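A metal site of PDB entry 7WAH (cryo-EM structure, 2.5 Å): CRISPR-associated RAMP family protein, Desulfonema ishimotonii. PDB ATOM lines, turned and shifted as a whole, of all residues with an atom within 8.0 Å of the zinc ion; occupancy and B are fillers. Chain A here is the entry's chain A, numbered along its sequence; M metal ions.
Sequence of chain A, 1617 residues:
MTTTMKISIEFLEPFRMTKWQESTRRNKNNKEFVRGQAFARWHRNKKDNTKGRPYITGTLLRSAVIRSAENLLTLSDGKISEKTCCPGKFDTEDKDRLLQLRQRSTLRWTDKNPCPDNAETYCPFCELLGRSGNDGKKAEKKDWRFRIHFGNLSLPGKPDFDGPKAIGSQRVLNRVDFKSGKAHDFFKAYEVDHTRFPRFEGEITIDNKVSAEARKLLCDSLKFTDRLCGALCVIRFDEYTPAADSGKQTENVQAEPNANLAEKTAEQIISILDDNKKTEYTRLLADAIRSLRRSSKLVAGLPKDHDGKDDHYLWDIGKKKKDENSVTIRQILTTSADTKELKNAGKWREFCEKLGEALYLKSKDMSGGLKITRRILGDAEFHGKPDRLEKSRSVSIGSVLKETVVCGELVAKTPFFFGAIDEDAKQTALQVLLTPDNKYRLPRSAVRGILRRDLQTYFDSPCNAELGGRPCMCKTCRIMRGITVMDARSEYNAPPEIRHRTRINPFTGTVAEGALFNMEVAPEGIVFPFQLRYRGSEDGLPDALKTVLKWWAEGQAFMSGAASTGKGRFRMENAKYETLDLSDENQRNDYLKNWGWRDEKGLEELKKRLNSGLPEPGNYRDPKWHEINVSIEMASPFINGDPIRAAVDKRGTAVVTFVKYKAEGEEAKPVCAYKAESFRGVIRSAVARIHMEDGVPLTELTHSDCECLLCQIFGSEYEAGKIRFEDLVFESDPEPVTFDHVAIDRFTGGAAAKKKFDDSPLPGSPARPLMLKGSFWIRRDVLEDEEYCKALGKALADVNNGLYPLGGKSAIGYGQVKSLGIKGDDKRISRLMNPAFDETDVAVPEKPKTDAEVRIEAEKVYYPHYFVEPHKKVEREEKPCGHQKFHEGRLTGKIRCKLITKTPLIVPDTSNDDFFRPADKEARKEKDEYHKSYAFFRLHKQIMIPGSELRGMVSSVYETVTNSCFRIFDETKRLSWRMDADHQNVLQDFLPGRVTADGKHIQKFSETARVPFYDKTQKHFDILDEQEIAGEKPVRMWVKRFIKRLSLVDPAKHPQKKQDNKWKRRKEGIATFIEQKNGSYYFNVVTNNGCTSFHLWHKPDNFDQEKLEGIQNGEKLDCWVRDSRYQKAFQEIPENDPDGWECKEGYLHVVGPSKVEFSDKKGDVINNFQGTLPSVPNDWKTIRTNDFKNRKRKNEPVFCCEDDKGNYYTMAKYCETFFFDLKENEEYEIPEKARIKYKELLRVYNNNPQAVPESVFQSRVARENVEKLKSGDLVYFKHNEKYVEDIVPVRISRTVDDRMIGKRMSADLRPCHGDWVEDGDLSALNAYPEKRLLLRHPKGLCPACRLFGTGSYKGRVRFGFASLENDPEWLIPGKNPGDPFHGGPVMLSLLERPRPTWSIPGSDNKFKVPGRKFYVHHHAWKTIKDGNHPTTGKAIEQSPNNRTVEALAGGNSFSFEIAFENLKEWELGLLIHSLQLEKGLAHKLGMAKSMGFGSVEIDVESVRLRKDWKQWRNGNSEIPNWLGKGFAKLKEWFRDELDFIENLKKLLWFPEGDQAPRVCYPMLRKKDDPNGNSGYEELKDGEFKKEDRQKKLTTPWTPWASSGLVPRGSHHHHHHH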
ATOM      1  N   THR A  84      26.348  -3.983 -19.515  1.00  0.00           N
ATOM      2  CA  THR A  84      27.238  -5.042 -19.041  1.00  0.00           C
ATOM      3  C   THR A  84      26.495  -5.851 -17.986  1.00  0.00           C
ATOM      4  O   THR A  84      25.958  -5.281 -17.018  1.00  0.00           O
ATOM      5  CB  THR A  84      28.524  -4.459 -18.454  1.00  0.00           C
ATOM      6  OG1 THR A  84      28.225  -3.723 -17.264  1.00  0.00           O
ATOM      7  CG2 THR A  84      29.185  -3.532 -19.453  1.00  0.00           C
ATOM      8  N   CYS A  85      26.462  -7.164 -18.154  1.00  0.00           N
ATOM      9  CA  CYS A  85      25.793  -8.038 -17.200  1.00  0.00           C
ATOM     10  C   CYS A  85      26.643  -8.223 -15.953  1.00  0.00           C
ATOM     11  O   CYS A  85      27.861  -8.046 -15.959  1.00  0.00           O
ATOM     12  CB  CYS A  85      25.492  -9.392 -17.823  1.00  0.00           C
ATOM     13  SG  CYS A  85      24.057  -9.414 -18.919  1.00  0.00           S
ATOM     14  N   CYS A  86      25.968  -8.582 -14.854  1.00  0.00           N
ATOM     15  CA  CYS A  86      26.623  -8.921 -13.604  1.00  0.00           C
ATOM     16  C   CYS A  86      27.118 -10.352 -13.700  1.00  0.00           C
ATOM     17  O   CYS A  86      26.769 -11.053 -14.670  1.00  0.00           O
ATOM     18  CB  CYS A  86      25.652  -8.734 -12.430  1.00  0.00           C
ATOM     19  SG  CYS A  86      24.609 -10.155 -12.074  1.00  0.00           S
ATOM     20  N   PRO A  87      27.939 -10.850 -12.762  1.00  0.00           N
ATOM     21  CA  PRO A  87      28.383 -12.244 -12.842  1.00  0.00           C
ATOM     22  C   PRO A  87      27.247 -13.256 -12.749  1.00  0.00           C
ATOM     23  O   PRO A  87      27.460 -14.438 -13.041  1.00  0.00           O
ATOM     24  CB  PRO A  87      29.342 -12.379 -11.660  1.00  0.00           C
ATOM     25  CG  PRO A  87      28.920 -11.325 -10.724  1.00  0.00           C
ATOM     26  CD  PRO A  87      28.536 -10.171 -11.592  1.00  0.00           C
ATOM     27  N   GLY A  88      26.057 -12.828 -12.351  1.00  0.00           N
ATOM     28  CA  GLY A  88      24.932 -13.726 -12.217  1.00  0.00           C
ATOM     29  C   GLY A  88      24.760 -14.196 -10.791  1.00  0.00           C
ATOM     30  O   GLY A  88      25.722 -14.354 -10.031  1.00  0.00           O
ATOM     31  N   LYS A  89      23.502 -14.415 -10.412  1.00  0.00           N
ATOM     32  CA  LYS A  89      23.175 -14.812  -9.054  1.00  0.00           C
ATOM     33  C   LYS A  89      22.588 -16.213  -9.069  1.00  0.00           C
ATOM     34  O   LYS A  89      21.467 -16.424  -9.558  1.00  0.00           O
ATOM     35  CB  LYS A  89      22.200 -13.826  -8.411  1.00  0.00           C
ATOM     36  CG  LYS A  89      21.765 -14.198  -7.010  1.00  0.00           C
ATOM     37  CD  LYS A  89      21.380 -12.978  -6.204  1.00  0.00           C
ATOM     38  CE  LYS A  89      20.715 -13.374  -4.896  1.00  0.00           C
ATOM     39  NZ  LYS A  89      21.540 -14.333  -4.125  1.00  0.00           N
ATOM     40  N   TRP A 109      32.689 -14.309 -16.265  1.00  0.00           N
ATOM     41  CA  TRP A 109      33.049 -13.320 -17.257  1.00  0.00           C
ATOM     42  C   TRP A 109      33.367 -11.951 -16.669  1.00  0.00           C
ATOM     43  O   TRP A 109      33.747 -11.047 -17.416  1.00  0.00           O
ATOM     44  CB  TRP A 109      31.934 -13.170 -18.299  1.00  0.00           C
ATOM     45  CG  TRP A 109      30.584 -12.914 -17.710  1.00  0.00           C
ATOM     46  CD1 TRP A 109      30.070 -11.706 -17.326  1.00  0.00           C
ATOM     47  CD2 TRP A 109      29.577 -13.891 -17.418  1.00  0.00           C
ATOM     48  NE1 TRP A 109      28.805 -11.870 -16.824  1.00  0.00           N
ATOM     49  CE2 TRP A 109      28.482 -13.205 -16.865  1.00  0.00           C
ATOM     50  CE3 TRP A 109      29.494 -15.279 -17.564  1.00  0.00           C
ATOM     51  CZ2 TRP A 109      27.309 -13.849 -16.464  1.00  0.00           C
ATOM     52  CZ3 TRP A 109      28.342 -15.920 -17.168  1.00  0.00           C
ATOM     53  CH2 TRP A 109      27.260 -15.209 -16.623  1.00  0.00           C
ATOM     54  N   ASN A 113      30.638  -7.660  -8.299  1.00  0.00           N
ATOM     55  CA  ASN A 113      29.692  -8.292  -7.399  1.00  0.00           C
ATOM     56  C   ASN A 113      28.357  -8.486  -8.104  1.00  0.00           C
ATOM     57  O   ASN A 113      27.983  -7.687  -8.959  1.00  0.00           O
ATOM     58  CB  ASN A 113      29.503  -7.434  -6.142  1.00  0.00           C
ATOM     59  CG  ASN A 113      28.730  -8.140  -5.048  1.00  0.00           C
ATOM     60  OD1 ASN A 113      29.310  -8.813  -4.206  1.00  0.00           O
ATOM     61  ND2 ASN A 113      27.410  -7.989  -5.066  1.00  0.00           N
ATOM     62  N   PRO A 114      27.623  -9.553  -7.783  1.00  0.00           N
ATOM     63  CA  PRO A 114      26.288  -9.723  -8.366  1.00  0.00           C
ATOM     64  C   PRO A 114      25.359  -8.587  -7.970  1.00  0.00           C
ATOM     65  O   PRO A 114      25.616  -7.830  -7.028  1.00  0.00           O
ATOM     66  CB  PRO A 114      25.812 -11.067  -7.787  1.00  0.00           C
ATOM     67  CG  PRO A 114      26.722 -11.346  -6.624  1.00  0.00           C
ATOM     68  CD  PRO A 114      28.030 -10.727  -6.995  1.00  0.00           C
ATOM     69  N   CYS A 115      24.270  -8.467  -8.718  1.00  0.00           N
ATOM     70  CA  CYS A 115      23.346  -7.367  -8.537  1.00  0.00           C
ATOM     71  C   CYS A 115      22.744  -7.391  -7.131  1.00  0.00           C
ATOM     72  O   CYS A 115      22.572  -8.468  -6.537  1.00  0.00           O
ATOM     73  CB  CYS A 115      22.227  -7.410  -9.586  1.00  0.00           C
ATOM     74  SG  CYS A 115      22.757  -6.946 -11.249  1.00  0.00           S
ATOM     75  N   PRO A 116      22.417  -6.232  -6.562  1.00  0.00           N
ATOM     76  CA  PRO A 116      21.841  -6.198  -5.214  1.00  0.00           C
ATOM     77  C   PRO A 116      20.510  -6.920  -5.159  1.00  0.00           C
ATOM     78  O   PRO A 116      19.775  -6.998  -6.152  1.00  0.00           O
ATOM     79  CB  PRO A 116      21.676  -4.693  -4.938  1.00  0.00           C
ATOM     80  CG  PRO A 116      22.629  -4.026  -5.865  1.00  0.00           C
ATOM     81  CD  PRO A 116      22.652  -4.883  -7.102  1.00  0.00           C
ATOM     82  N   THR A 121      16.806  -1.106 -10.724  1.00  0.00           N
ATOM     83  CA  THR A 121      16.958  -1.752 -12.019  1.00  0.00           C
ATOM     84  C   THR A 121      17.879  -2.954 -11.889  1.00  0.00           C
ATOM     85  O   THR A 121      18.770  -2.994 -11.026  1.00  0.00           O
ATOM     86  CB  THR A 121      17.511  -0.787 -13.080  1.00  0.00           C
ATOM     87  OG1 THR A 121      17.679  -1.481 -14.314  1.00  0.00           O
ATOM     88  CG2 THR A 121      18.844  -0.205 -12.640  1.00  0.00           C
ATOM     89  N   TYR A 122      17.660  -3.944 -12.747  1.00  0.00           N
ATOM     90  CA  TYR A 122      18.455  -5.165 -12.775  1.00  0.00           C
ATOM     91  C   TYR A 122      19.118  -5.311 -14.142  1.00  0.00           C
ATOM     92  O   TYR A 122      18.583  -4.846 -15.155  1.00  0.00           O
ATOM     93  CB  TYR A 122      17.609  -6.408 -12.476  1.00  0.00           C
ATOM     94  CG  TYR A 122      17.029  -6.439 -11.080  1.00  0.00           C
ATOM     95  CD1 TYR A 122      15.805  -5.835 -10.812  1.00  0.00           C
ATOM     96  CD2 TYR A 122      17.699  -7.076 -10.046  1.00  0.00           C
ATOM     97  CE1 TYR A 122      15.268  -5.866  -9.540  1.00  0.00           C
ATOM     98  CE2 TYR A 122      17.171  -7.108  -8.772  1.00  0.00           C
ATOM     99  CZ  TYR A 122      15.952  -6.496  -8.523  1.00  0.00           C
ATOM    100  OH  TYR A 122      15.424  -6.528  -7.249  1.00  0.00           O
ATOM    101  N   CYS A 123      20.271  -5.978 -14.163  1.00  0.00           N
ATOM    102  CA  CYS A 123      20.941  -6.276 -15.406  1.00  0.00           C
ATOM    103  C   CYS A 123      20.103  -7.260 -16.226  1.00  0.00           C
ATOM    104  O   CYS A 123      19.245  -7.960 -15.671  1.00  0.00           O
ATOM    105  CB  CYS A 123      22.324  -6.852 -15.138  1.00  0.00           C
ATOM    106  SG  CYS A 123      22.335  -8.589 -14.659  1.00  0.00           S
ATOM    107  N   PRO A 124      20.325  -7.320 -17.539  1.00  0.00           N
ATOM    108  CA  PRO A 124      19.543  -8.259 -18.362  1.00  0.00           C
ATOM    109  C   PRO A 124      19.673  -9.701 -17.907  1.00  0.00           C
ATOM    110  O   PRO A 124      18.706 -10.467 -18.026  1.00  0.00           O
ATOM    111  CB  PRO A 124      20.119  -8.048 -19.770  1.00  0.00           C
ATOM    112  CG  PRO A 124      20.652  -6.664 -19.741  1.00  0.00           C
ATOM    113  CD  PRO A 124      21.175  -6.447 -18.366  1.00  0.00           C
ATOM    114  N   PHE A 125      20.836 -10.104 -17.410  1.00  0.00           N
ATOM    115  CA  PHE A 125      21.011 -11.483 -16.952  1.00  0.00           C
ATOM    116  C   PHE A 125      20.118 -11.778 -15.749  1.00  0.00           C
ATOM    117  O   PHE A 125      19.509 -12.849 -15.669  1.00  0.00           O
ATOM    118  CB  PHE A 125      22.479 -11.740 -16.615  1.00  0.00           C
ATOM    119  CG  PHE A 125      22.825 -13.199 -16.521  1.00  0.00           C
ATOM    120  CD1 PHE A 125      22.399 -14.086 -17.489  1.00  0.00           C
ATOM    121  CD2 PHE A 125      23.597 -13.678 -15.475  1.00  0.00           C
ATOM    122  CE1 PHE A 125      22.716 -15.431 -17.407  1.00  0.00           C
ATOM    123  CE2 PHE A 125      23.924 -15.015 -15.387  1.00  0.00           C
ATOM    124  CZ  PHE A 125      23.488 -15.892 -16.353  1.00  0.00           C
ATOM    125  N   CYS A 126      20.022 -10.838 -14.803  1.00  0.00           N
ATOM    126  CA  CYS A 126      19.147 -11.034 -13.653  1.00  0.00           C
ATOM    127  C   CYS A 126      17.679 -11.054 -14.055  1.00  0.00           C
ATOM    128  O   CYS A 126      16.885 -11.804 -13.486  1.00  0.00           O
ATOM    129  CB  CYS A 126      19.400  -9.954 -12.605  1.00  0.00           C
ATOM    130  SG  CYS A 126      20.852 -10.241 -11.573  1.00  0.00           S
ATOM    131  N   GLU A 127      17.299 -10.233 -15.035  1.00  0.00           N
ATOM    132  CA  GLU A 127      15.940 -10.272 -15.545  1.00  0.00           C
ATOM    133  C   GLU A 127      15.635 -11.614 -16.196  1.00  0.00           C
ATOM    134  O   GLU A 127      14.540 -12.171 -16.018  1.00  0.00           O
ATOM    135  CB  GLU A 127      15.711  -9.137 -16.544  1.00  0.00           C
ATOM    136  CG  GLU A 127      16.041  -7.754 -16.014  1.00  0.00           C
ATOM    137  CD  GLU A 127      15.737  -6.653 -17.011  1.00  0.00           C
ATOM    138  OE1 GLU A 127      14.641  -6.692 -17.620  1.00  0.00           O
ATOM    139  OE2 GLU A 127      16.585  -5.765 -17.197  1.00  0.00           O
ATOM    140  N   LEU A 129      17.095 -14.452 -15.419  1.00  0.00           N
ATOM    141  CA  LEU A 129      17.004 -15.411 -14.322  1.00  0.00           C
ATOM    142  C   LEU A 129      15.635 -15.333 -13.649  1.00  0.00           C
ATOM    143  O   LEU A 129      15.098 -16.363 -13.213  1.00  0.00           O
ATOM    144  CB  LEU A 129      18.115 -15.157 -13.306  1.00  0.00           C
ATOM    145  CG  LEU A 129      19.542 -15.437 -13.766  1.00  0.00           C
ATOM    146  CD1 LEU A 129      20.531 -15.092 -12.658  1.00  0.00           C
ATOM    147  CD2 LEU A 129      19.697 -16.880 -14.185  1.00  0.00           C
ATOM    148  N   ARG A 131      14.928 -12.542 -11.270  1.00  0.00           N
ATOM    149  CA  ARG A 131      14.996 -11.752 -10.055  1.00  0.00           C
ATOM    150  C   ARG A 131      14.204 -10.453 -10.180  1.00  0.00           C
ATOM    151  O   ARG A 131      13.624  -9.980  -9.187  1.00  0.00           O
ATOM    152  CB  ARG A 131      16.444 -11.440  -9.696  1.00  0.00           C
ATOM    153  CG  ARG A 131      17.289 -12.668  -9.383  1.00  0.00           C
ATOM    154  CD  ARG A 131      18.712 -12.252  -9.063  1.00  0.00           C
ATOM    155  NE  ARG A 131      18.737 -11.194  -8.062  1.00  0.00           N
ATOM    156  CZ  ARG A 131      19.789 -10.438  -7.795  1.00  0.00           C
ATOM    157  NH1 ARG A 131      20.934 -10.590  -8.449  1.00  0.00           N
ATOM    158  NH2 ARG A 131      19.701  -9.512  -6.843  1.00  0.00           N
HETATM  159 ZN    ZN M   1      22.628  -8.981 -12.387  1.00  0.00          ZN
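SG of Cys 86 sits close to N of Gly 88 (3.1 Å). The backbone carbonyl oxygen (O) of Cys 86 sits at hydrogen-bond distance from the indole nitrogen (NE1) of Trp 109, at 3.1 Å. The side-chain sulfur (SG) of Cys 123 lies close to the backbone NH (N) of Phe 125 (3.5 Å). O of Cys 126 is in hydrogen-bond range of N of Arg 131, at 3.0 Å. The backbone carbonyl oxygen (O) of Cys 115 lies within hydrogen-bond range of the guanidinium group (NH2) of Arg 131, 3.1 Å away.
Four residues have an atom within 4 Å of the zinc ion: Cys 86, Cys 115, Cys 123 and Cys 126.
The zinc ion is bound by SG of Cys 86 (2.3 Å), SG of Cys 123 (2.3 Å), SG of Cys 126 (2.3 Å) and SG of Cys 115 (2.3 Å).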
